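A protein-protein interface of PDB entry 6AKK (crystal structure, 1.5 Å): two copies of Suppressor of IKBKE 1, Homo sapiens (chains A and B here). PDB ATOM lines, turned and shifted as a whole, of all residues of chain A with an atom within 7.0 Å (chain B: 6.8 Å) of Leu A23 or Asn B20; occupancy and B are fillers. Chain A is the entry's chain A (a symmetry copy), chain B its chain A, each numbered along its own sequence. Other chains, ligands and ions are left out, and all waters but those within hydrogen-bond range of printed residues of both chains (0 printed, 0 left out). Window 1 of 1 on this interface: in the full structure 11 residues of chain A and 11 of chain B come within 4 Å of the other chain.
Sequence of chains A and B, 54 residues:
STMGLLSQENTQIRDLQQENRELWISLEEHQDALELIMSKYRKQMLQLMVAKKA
Among the printed residues, pairs that only touch across the chains: Leu A16 with Leu B16 (3.97 Å), Asn A20 with Leu B23 (3.5 Å), Leu A23 with Asn B20 (3.5 Å), Leu A23 with Leu B23 (3.7 Å), Leu A23 with Trp B24 (3.9 Å), Leu A23 with Leu B27 (3.6 Å), Trp A24 with Leu B23 (3.9 Å), Leu A27 with Leu B23 (3.6 Å) and Leu A27 with Leu B27 (3.7 Å).
Of the printed residues of chain B, Leu A23 touches Asn B20, Leu B23, Trp B24 and Leu B27.
Of the printed residues of chain A, Asn B20 touches Leu A23 (3.5 Å).
Printed residues of chain B within 4 Å of Asn A20: Leu B23.
Printed residues of chain A within 4 Å of Trp B24: Leu A23 (3.9 Å).
Of the printed residues of chain B, Trp A24 touches Leu B23 (3.9 Å).
The nearest printed residue of chain A that does not touch Asn B20 is Glu A19 (4.3 Å).
The nearest printed residue of chain B that does not touch Trp A24 is Leu B27 (6.4 Å).
Hydrophobic or aromatic side chains of chain A that line the printed part of chain B: Leu A16, Leu A23, Trp A24 and Leu A27.
Of the 12 printed residues of chain B, 5 touch a printed residue of chain A.
Among the printed residues, 9 pairs touch across the chains.
Leu B23 touches its own counterpart, Leu A23.
Leu A23 touches Trp B24, and with the chains exchanged Trp A24 touches Leu B23.
Leu A23 touches Leu B27, and with the chains exchanged Leu A27 touches Leu B23.
Leu B27 touches its own counterpart, Leu A27.
Positions printed for both chains: 16, 18, 19, 20, 21, 22, 23, 24, 25 and 27.
Of the 9 pairs that touch across the chains among the printed residues, 9 have their exchanged pair printed and touching as well.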
ATOM      1  N   LEU A  16     -22.192 -18.333  22.464  1.00  0.00           N
ATOM      2  CA  LEU A  16     -21.894 -17.159  23.284  1.00  0.00           C
ATOM      3  C   LEU A  16     -20.421 -17.084  23.658  1.00  0.00           C
ATOM      4  O   LEU A  16     -19.867 -15.983  23.765  1.00  0.00           O
ATOM      5  CB  LEU A  16     -22.749 -17.158  24.552  1.00  0.00           C
ATOM      6  CG  LEU A  16     -24.229 -16.808  24.385  1.00  0.00           C
ATOM      7  CD1 LEU A  16     -25.064 -17.313  25.563  1.00  0.00           C
ATOM      8  CD2 LEU A  16     -24.382 -15.311  24.228  1.00  0.00           C
ATOM      9  N   GLN A  18     -17.987 -18.030  21.766  1.00  0.00           N
ATOM     10  CA  GLN A  18     -17.308 -17.591  20.524  1.00  0.00           C
ATOM     11  C   GLN A  18     -17.517 -16.087  20.384  1.00  0.00           C
ATOM     12  O   GLN A  18     -16.587 -15.439  20.037  1.00  0.00           O
ATOM     13  CB  GLN A  18     -17.872 -18.367  19.326  1.00  0.00           C
ATOM     14  CG  GLN A  18     -17.160 -18.084  18.010  1.00  0.00           C
ATOM     15  CD  GLN A  18     -15.790 -18.709  17.881  1.00  0.00           C
ATOM     16  OE1 GLN A  18     -15.211 -19.255  18.812  1.00  0.00           O
ATOM     17  NE2 GLN A  18     -15.234 -18.641  16.694  1.00  0.00           N
ATOM     18  N   GLU A  19     -18.709 -15.599  20.649  1.00  0.00           N
ATOM     19  CA  GLU A  19     -18.954 -14.158  20.626  1.00  0.00           C
ATOM     20  C   GLU A  19     -18.084 -13.438  21.649  1.00  0.00           C
ATOM     21  O   GLU A  19     -17.459 -12.420  21.343  1.00  0.00           O
ATOM     22  CB  GLU A  19     -20.436 -13.876  20.898  1.00  0.00           C
ATOM     23  N   ASN A  20     -18.083 -13.946  22.890  1.00  0.00           N
ATOM     24  CA  ASN A  20     -17.209 -13.445  23.949  1.00  0.00           C
ATOM     25  C   ASN A  20     -15.785 -13.277  23.442  1.00  0.00           C
ATOM     26  O   ASN A  20     -15.172 -12.210  23.590  1.00  0.00           O
ATOM     27  CB  ASN A  20     -17.250 -14.415  25.139  1.00  0.00           C
ATOM     28  CG  ASN A  20     -16.343 -13.995  26.292  1.00  0.00           C
ATOM     29  OD1 ASN A  20     -16.777 -13.293  27.203  1.00  0.00           O
ATOM     30  ND2 ASN A  20     -15.091 -14.445  26.270  1.00  0.00           N
ATOM     31  N   ARG A  21     -15.256 -14.327  22.817  1.00  0.00           N
ATOM     32  CA  ARG A  21     -13.876 -14.306  22.346  1.00  0.00           C
ATOM     33  C   ARG A  21     -13.686 -13.241  21.277  1.00  0.00           C
ATOM     34  O   ARG A  21     -12.645 -12.576  21.234  1.00  0.00           O
ATOM     35  CB  ARG A  21     -13.475 -15.680  21.812  1.00  0.00           C
ATOM     36  CG  ARG A  21     -13.051 -16.656  22.907  1.00  0.00           C
ATOM     37  CD  ARG A  21     -12.437 -17.933  22.341  1.00  0.00           C
ATOM     38  NE  ARG A  21     -13.382 -18.725  21.566  1.00  0.00           N
ATOM     39  CZ  ARG A  21     -14.138 -19.688  22.086  1.00  0.00           C
ATOM     40  NH1 ARG A  21     -14.056 -19.968  23.379  1.00  0.00           N
ATOM     41  NH2 ARG A  21     -14.980 -20.356  21.323  1.00  0.00           N
ATOM     42  N   GLU A  22     -14.683 -13.061  20.409  1.00  0.00           N
ATOM     43  CA  GLU A  22     -14.558 -12.070  19.346  1.00  0.00           C
ATOM     44  C   GLU A  22     -14.554 -10.654  19.904  1.00  0.00           C
ATOM     45  O   GLU A  22     -13.844  -9.779  19.386  1.00  0.00           O
ATOM     46  CB  GLU A  22     -15.684 -12.246  18.329  1.00  0.00           C
ATOM     47  CG  GLU A  22     -15.339 -11.741  16.945  1.00  0.00           C
ATOM     48  CD  GLU A  22     -14.272 -12.574  16.253  1.00  0.00           C
ATOM     49  OE1 GLU A  22     -13.966 -13.698  16.717  1.00  0.00           O
ATOM     50  OE2 GLU A  22     -13.757 -12.122  15.217  1.00  0.00           O
ATOM     51  N   LEU A  23     -15.347 -10.404  20.954  1.00  0.00           N
ATOM     52  CA  LEU A  23     -15.338  -9.100  21.608  1.00  0.00           C
ATOM     53  C   LEU A  23     -13.981  -8.808  22.235  1.00  0.00           C
ATOM     54  O   LEU A  23     -13.435  -7.703  22.078  1.00  0.00           O
ATOM     55  CB  LEU A  23     -16.449  -9.051  22.661  1.00  0.00           C
ATOM     56  CG  LEU A  23     -17.852  -9.029  22.070  1.00  0.00           C
ATOM     57  CD1 LEU A  23     -18.892  -9.344  23.143  1.00  0.00           C
ATOM     58  CD2 LEU A  23     -18.133  -7.690  21.417  1.00  0.00           C
ATOM     59  N   TRP A  24     -13.425  -9.790  22.954  1.00  0.00           N
ATOM     60  CA  TRP A  24     -12.083  -9.669  23.526  1.00  0.00           C
ATOM     61  C   TRP A  24     -11.027  -9.408  22.458  1.00  0.00           C
ATOM     62  O   TRP A  24     -10.109  -8.607  22.672  1.00  0.00           O
ATOM     63  CB  TRP A  24     -11.724 -10.939  24.309  1.00  0.00           C
ATOM     64  CG  TRP A  24     -12.056 -10.859  25.748  1.00  0.00           C
ATOM     65  CD1 TRP A  24     -12.968 -11.616  26.420  1.00  0.00           C
ATOM     66  CD2 TRP A  24     -11.483  -9.969  26.715  1.00  0.00           C
ATOM     67  NE1 TRP A  24     -13.012 -11.247  27.743  1.00  0.00           N
ATOM     68  CE2 TRP A  24     -12.103 -10.242  27.950  1.00  0.00           C
ATOM     69  CE3 TRP A  24     -10.509  -8.972  26.660  1.00  0.00           C
ATOM     70  CZ2 TRP A  24     -11.780  -9.556  29.113  1.00  0.00           C
ATOM     71  CZ3 TRP A  24     -10.187  -8.293  27.824  1.00  0.00           C
ATOM     72  CH2 TRP A  24     -10.824  -8.585  29.028  1.00  0.00           C
ATOM     73  N   ILE A  25     -11.088 -10.117  21.329  1.00  0.00           N
ATOM     74  CA  ILE A  25     -10.114  -9.875  20.271  1.00  0.00           C
ATOM     75  C   ILE A  25     -10.252  -8.453  19.747  1.00  0.00           C
ATOM     76  O   ILE A  25      -9.253  -7.767  19.489  1.00  0.00           O
ATOM     77  CB  ILE A  25     -10.266 -10.919  19.154  1.00  0.00           C
ATOM     78  CG1 ILE A  25      -9.808 -12.272  19.687  1.00  0.00           C
ATOM     79  CG2 ILE A  25      -9.470 -10.523  17.909  1.00  0.00           C
ATOM     80  CD1 ILE A  25     -10.271 -13.419  18.860  1.00  0.00           C
ATOM     81  N   SER A  26     -11.489  -7.983  19.596  1.00  0.00           N
ATOM     82  CA  SER A  26     -11.692  -6.593  19.190  1.00  0.00           C
ATOM     83  C   SER A  26     -11.047  -5.625  20.176  1.00  0.00           C
ATOM     84  O   SER A  26     -10.386  -4.660  19.767  1.00  0.00           O
ATOM     85  CB  SER A  26     -13.186  -6.303  19.071  1.00  0.00           C
ATOM     86  OG  SER A  26     -13.772  -7.152  18.111  1.00  0.00           O
ATOM     87  N   LEU A  27     -11.210  -5.866  21.481  1.00  0.00           N
ATOM     88  CA  LEU A  27     -10.582  -4.991  22.471  1.00  0.00           C
ATOM     89  C   LEU A  27      -9.066  -5.100  22.405  1.00  0.00           C
ATOM     90  O   LEU A  27      -8.357  -4.087  22.512  1.00  0.00           O
ATOM     91  CB  LEU A  27     -11.080  -5.345  23.876  1.00  0.00           C
ATOM     92  CG  LEU A  27     -12.534  -4.978  24.187  1.00  0.00           C
ATOM     93  CD1 LEU A  27     -13.114  -5.832  25.309  1.00  0.00           C
ATOM     94  CD2 LEU A  27     -12.605  -3.509  24.567  1.00  0.00           C
ATOM     95  N   GLU A  28      -8.546  -6.319  22.218  1.00  0.00           N
ATOM     96  CA  GLU A  28      -7.101  -6.521  22.247  1.00  0.00           C
ATOM     97  C   GLU A  28      -6.435  -5.910  21.017  1.00  0.00           C
ATOM     98  O   GLU A  28      -5.376  -5.275  21.115  1.00  0.00           O
ATOM     99  CB  GLU A  28      -6.804  -8.019  22.362  1.00  0.00           C
ATOM    100  CG  GLU A  28      -7.196  -8.575  23.718  1.00  0.00           C
ATOM    101  CD  GLU A  28      -7.387 -10.087  23.716  1.00  0.00           C
ATOM    102  OE1 GLU A  28      -7.348 -10.718  22.634  1.00  0.00           O
ATOM    103  OE2 GLU A  28      -7.559 -10.644  24.815  1.00  0.00           O
ATOM    104  N   GLU A  29      -7.048  -6.071  19.849  1.00  0.00           N
ATOM    105  CA  GLU A  29      -6.469  -5.510  18.637  1.00  0.00           C
ATOM    106  C   GLU A  29      -6.412  -3.995  18.722  1.00  0.00           C
ATOM    107  O   GLU A  29      -5.395  -3.390  18.376  1.00  0.00           O
ATOM    108  CB  GLU A  29      -7.279  -5.966  17.426  1.00  0.00           C
ATOM    109  CG  GLU A  29      -6.788  -5.399  16.110  1.00  0.00           C
ATOM    110  CD  GLU A  29      -5.463  -5.999  15.675  1.00  0.00           C
ATOM    111  OE1 GLU A  29      -5.115  -7.101  16.156  1.00  0.00           O
ATOM    112  OE2 GLU A  29      -4.773  -5.364  14.849  1.00  0.00           O
ATOM    113  N   ASP B  15     -25.301 -15.810  32.485  1.00  0.00           N
ATOM    114  CA  ASP B  15     -24.005 -15.266  32.884  1.00  0.00           C
ATOM    115  C   ASP B  15     -23.206 -14.805  31.670  1.00  0.00           C
ATOM    116  O   ASP B  15     -22.629 -13.710  31.675  1.00  0.00           O
ATOM    117  CB  ASP B  15     -23.214 -16.309  33.669  1.00  0.00           C
ATOM    118  CG  ASP B  15     -23.261 -16.076  35.164  1.00  0.00           C
ATOM    119  OD1 ASP B  15     -22.843 -14.985  35.613  1.00  0.00           O
ATOM    120  OD2 ASP B  15     -23.713 -16.986  35.890  1.00  0.00           O
ATOM    121  N   LEU B  16     -23.152 -15.635  30.624  1.00  0.00           N
ATOM    122  CA  LEU B  16     -22.429 -15.256  29.410  1.00  0.00           C
ATOM    123  C   LEU B  16     -23.069 -14.064  28.714  1.00  0.00           C
ATOM    124  O   LEU B  16     -22.360 -13.242  28.121  1.00  0.00           O
ATOM    125  CB  LEU B  16     -22.348 -16.436  28.440  1.00  0.00           C
ATOM    126  CG  LEU B  16     -21.377 -17.561  28.804  1.00  0.00           C
ATOM    127  CD1 LEU B  16     -21.730 -18.864  28.084  1.00  0.00           C
ATOM    128  CD2 LEU B  16     -19.963 -17.137  28.475  1.00  0.00           C
ATOM    129  N   GLN B  17     -24.401 -13.947  28.769  1.00  0.00           N
ATOM    130  CA  GLN B  17     -25.052 -12.790  28.164  1.00  0.00           C
ATOM    131  C   GLN B  17     -24.703 -11.514  28.920  1.00  0.00           C
ATOM    132  O   GLN B  17     -24.571 -10.449  28.311  1.00  0.00           O
ATOM    133  CB  GLN B  17     -26.566 -13.001  28.129  1.00  0.00           C
ATOM    134  CG  GLN B  17     -27.015 -14.015  27.088  1.00  0.00           C
ATOM    135  CD  GLN B  17     -28.461 -14.464  27.265  1.00  0.00           C
ATOM    136  OE1 GLN B  17     -29.028 -14.414  28.369  1.00  0.00           O
ATOM    137  NE2 GLN B  17     -29.066 -14.926  26.173  1.00  0.00           N
ATOM    138  N   GLN B  18     -24.509 -11.603  30.223  1.00  0.00           N
ATOM    139  CA  GLN B  18     -24.134 -10.438  31.058  1.00  0.00           C
ATOM    140  C   GLN B  18     -22.693 -10.066  30.723  1.00  0.00           C
ATOM    141  O   GLN B  18     -22.440  -8.914  30.614  1.00  0.00           O
ATOM    142  CB  GLN B  18     -24.310 -10.789  32.542  1.00  0.00           C
ATOM    143  CG  GLN B  18     -24.070  -9.623  33.491  1.00  0.00           C
ATOM    144  CD  GLN B  18     -25.170  -8.586  33.515  1.00  0.00           C
ATOM    145  OE1 GLN B  18     -26.102  -8.577  32.721  1.00  0.00           O
ATOM    146  NE2 GLN B  18     -25.081  -7.673  34.454  1.00  0.00           N
ATOM    147  N   GLU B  19     -21.819 -11.039  30.581  1.00  0.00           N
ATOM    148  CA  GLU B  19     -20.445 -10.760  30.168  1.00  0.00           C
ATOM    149  C   GLU B  19     -20.409 -10.100  28.796  1.00  0.00           C
ATOM    150  O   GLU B  19     -19.711  -9.104  28.591  1.00  0.00           O
ATOM    151  CB  GLU B  19     -19.631 -12.060  30.154  1.00  0.00           C
ATOM    152  N   ASN B  20     -21.131 -10.691  27.833  1.00  0.00           N
ATOM    153  CA  ASN B  20     -21.297 -10.113  26.501  1.00  0.00           C
ATOM    154  C   ASN B  20     -21.639  -8.634  26.590  1.00  0.00           C
ATOM    155  O   ASN B  20     -20.994  -7.786  25.957  1.00  0.00           O
ATOM    156  CB  ASN B  20     -22.396 -10.880  25.750  1.00  0.00           C
ATOM    157  CG  ASN B  20     -22.668 -10.332  24.352  1.00  0.00           C
ATOM    158  OD1 ASN B  20     -22.070 -10.785  23.378  1.00  0.00           O
ATOM    159  ND2 ASN B  20     -23.588  -9.376  24.246  1.00  0.00           N
ATOM    160  N   ARG B  21     -22.646  -8.312  27.400  1.00  0.00           N
ATOM    161  CA  ARG B  21     -23.106  -6.933  27.516  1.00  0.00           C
ATOM    162  C   ARG B  21     -22.013  -6.045  28.090  1.00  0.00           C
ATOM    163  O   ARG B  21     -21.860  -4.892  27.672  1.00  0.00           O
ATOM    164  CB  ARG B  21     -24.364  -6.863  28.380  1.00  0.00           C
ATOM    165  CG  ARG B  21     -25.645  -7.191  27.616  1.00  0.00           C
ATOM    166  CD  ARG B  21     -26.900  -6.891  28.429  1.00  0.00           C
ATOM    167  NE  ARG B  21     -27.023  -7.726  29.617  1.00  0.00           N
ATOM    168  CZ  ARG B  21     -27.665  -8.890  29.636  1.00  0.00           C
ATOM    169  NH1 ARG B  21     -28.233  -9.351  28.531  1.00  0.00           N
ATOM    170  NH2 ARG B  21     -27.725  -9.596  30.747  1.00  0.00           N
ATOM    171  N   GLU B  22     -21.240  -6.566  29.044  1.00  0.00           N
ATOM    172  CA  GLU B  22     -20.186  -5.761  29.652  1.00  0.00           C
ATOM    173  C   GLU B  22     -19.069  -5.469  28.661  1.00  0.00           C
ATOM    174  O   GLU B  22     -18.485  -4.376  28.680  1.00  0.00           O
ATOM    175  CB  GLU B  22     -19.638  -6.465  30.892  1.00  0.00           C
ATOM    176  CG  GLU B  22     -19.032  -5.523  31.909  1.00  0.00           C
ATOM    177  CD  GLU B  22     -20.061  -4.632  32.587  1.00  0.00           C
ATOM    178  OE1 GLU B  22     -21.282  -4.900  32.475  1.00  0.00           O
ATOM    179  OE2 GLU B  22     -19.652  -3.676  33.266  1.00  0.00           O
ATOM    180  N   LEU B  23     -18.747  -6.438  27.793  1.00  0.00           N
ATOM    181  CA  LEU B  23     -17.751  -6.212  26.752  1.00  0.00           C
ATOM    182  C   LEU B  23     -18.208  -5.134  25.777  1.00  0.00           C
ATOM    183  O   LEU B  23     -17.434  -4.229  25.425  1.00  0.00           O
ATOM    184  CB  LEU B  23     -17.472  -7.527  26.019  1.00  0.00           C
ATOM    185  CG  LEU B  23     -16.728  -8.552  26.865  1.00  0.00           C
ATOM    186  CD1 LEU B  23     -16.803  -9.936  26.222  1.00  0.00           C
ATOM    187  CD2 LEU B  23     -15.287  -8.126  27.070  1.00  0.00           C
ATOM    188  N   TRP B  24     -19.466  -5.220  25.329  1.00  0.00           N
ATOM    189  CA  TRP B  24     -20.055  -4.195  24.467  1.00  0.00           C
ATOM    190  C   TRP B  24     -20.035  -2.817  25.120  1.00  0.00           C
ATOM    191  O   TRP B  24     -19.767  -1.813  24.448  1.00  0.00           O
ATOM    192  CB  TRP B  24     -21.497  -4.573  24.102  1.00  0.00           C
ATOM    193  CG  TRP B  24     -21.606  -5.325  22.833  1.00  0.00           C
ATOM    194  CD1 TRP B  24     -22.035  -6.609  22.678  1.00  0.00           C
ATOM    195  CD2 TRP B  24     -21.282  -4.850  21.520  1.00  0.00           C
ATOM    196  NE1 TRP B  24     -21.986  -6.972  21.353  1.00  0.00           N
ATOM    197  CE2 TRP B  24     -21.534  -5.904  20.622  1.00  0.00           C
ATOM    198  CE3 TRP B  24     -20.806  -3.639  21.016  1.00  0.00           C
ATOM    199  CZ2 TRP B  24     -21.328  -5.784  19.254  1.00  0.00           C
ATOM    200  CZ3 TRP B  24     -20.605  -3.522  19.650  1.00  0.00           C
ATOM    201  CH2 TRP B  24     -20.860  -4.588  18.790  1.00  0.00           C
ATOM    202  N   ILE B  25     -20.380  -2.728  26.405  1.00  0.00           N
ATOM    203  CA  ILE B  25     -20.344  -1.431  27.074  1.00  0.00           C
ATOM    204  C   ILE B  25     -18.920  -0.895  27.102  1.00  0.00           C
ATOM    205  O   ILE B  25     -18.683   0.300  26.883  1.00  0.00           O
ATOM    206  CB  ILE B  25     -20.948  -1.538  28.483  1.00  0.00           C
ATOM    207  CG1 ILE B  25     -22.449  -1.773  28.352  1.00  0.00           C
ATOM    208  CG2 ILE B  25     -20.660  -0.284  29.309  1.00  0.00           C
ATOM    209  CD1 ILE B  25     -23.077  -2.286  29.599  1.00  0.00           C
ATOM    210  N   LEU B  27     -16.629  -1.453  24.853  1.00  0.00           N
ATOM    211  CA  LEU B  27     -16.346  -0.941  23.512  1.00  0.00           C
ATOM    212  C   LEU B  27     -17.068   0.376  23.272  1.00  0.00           C
ATOM    213  O   LEU B  27     -16.503   1.304  22.672  1.00  0.00           O
ATOM    214  CB  LEU B  27     -16.759  -1.974  22.458  1.00  0.00           C
ATOM    215  CG  LEU B  27     -15.891  -3.232  22.373  1.00  0.00           C
ATOM    216  CD1 LEU B  27     -16.645  -4.410  21.766  1.00  0.00           C
ATOM    217  CD2 LEU B  27     -14.655  -2.928  21.544  1.00  0.00           C
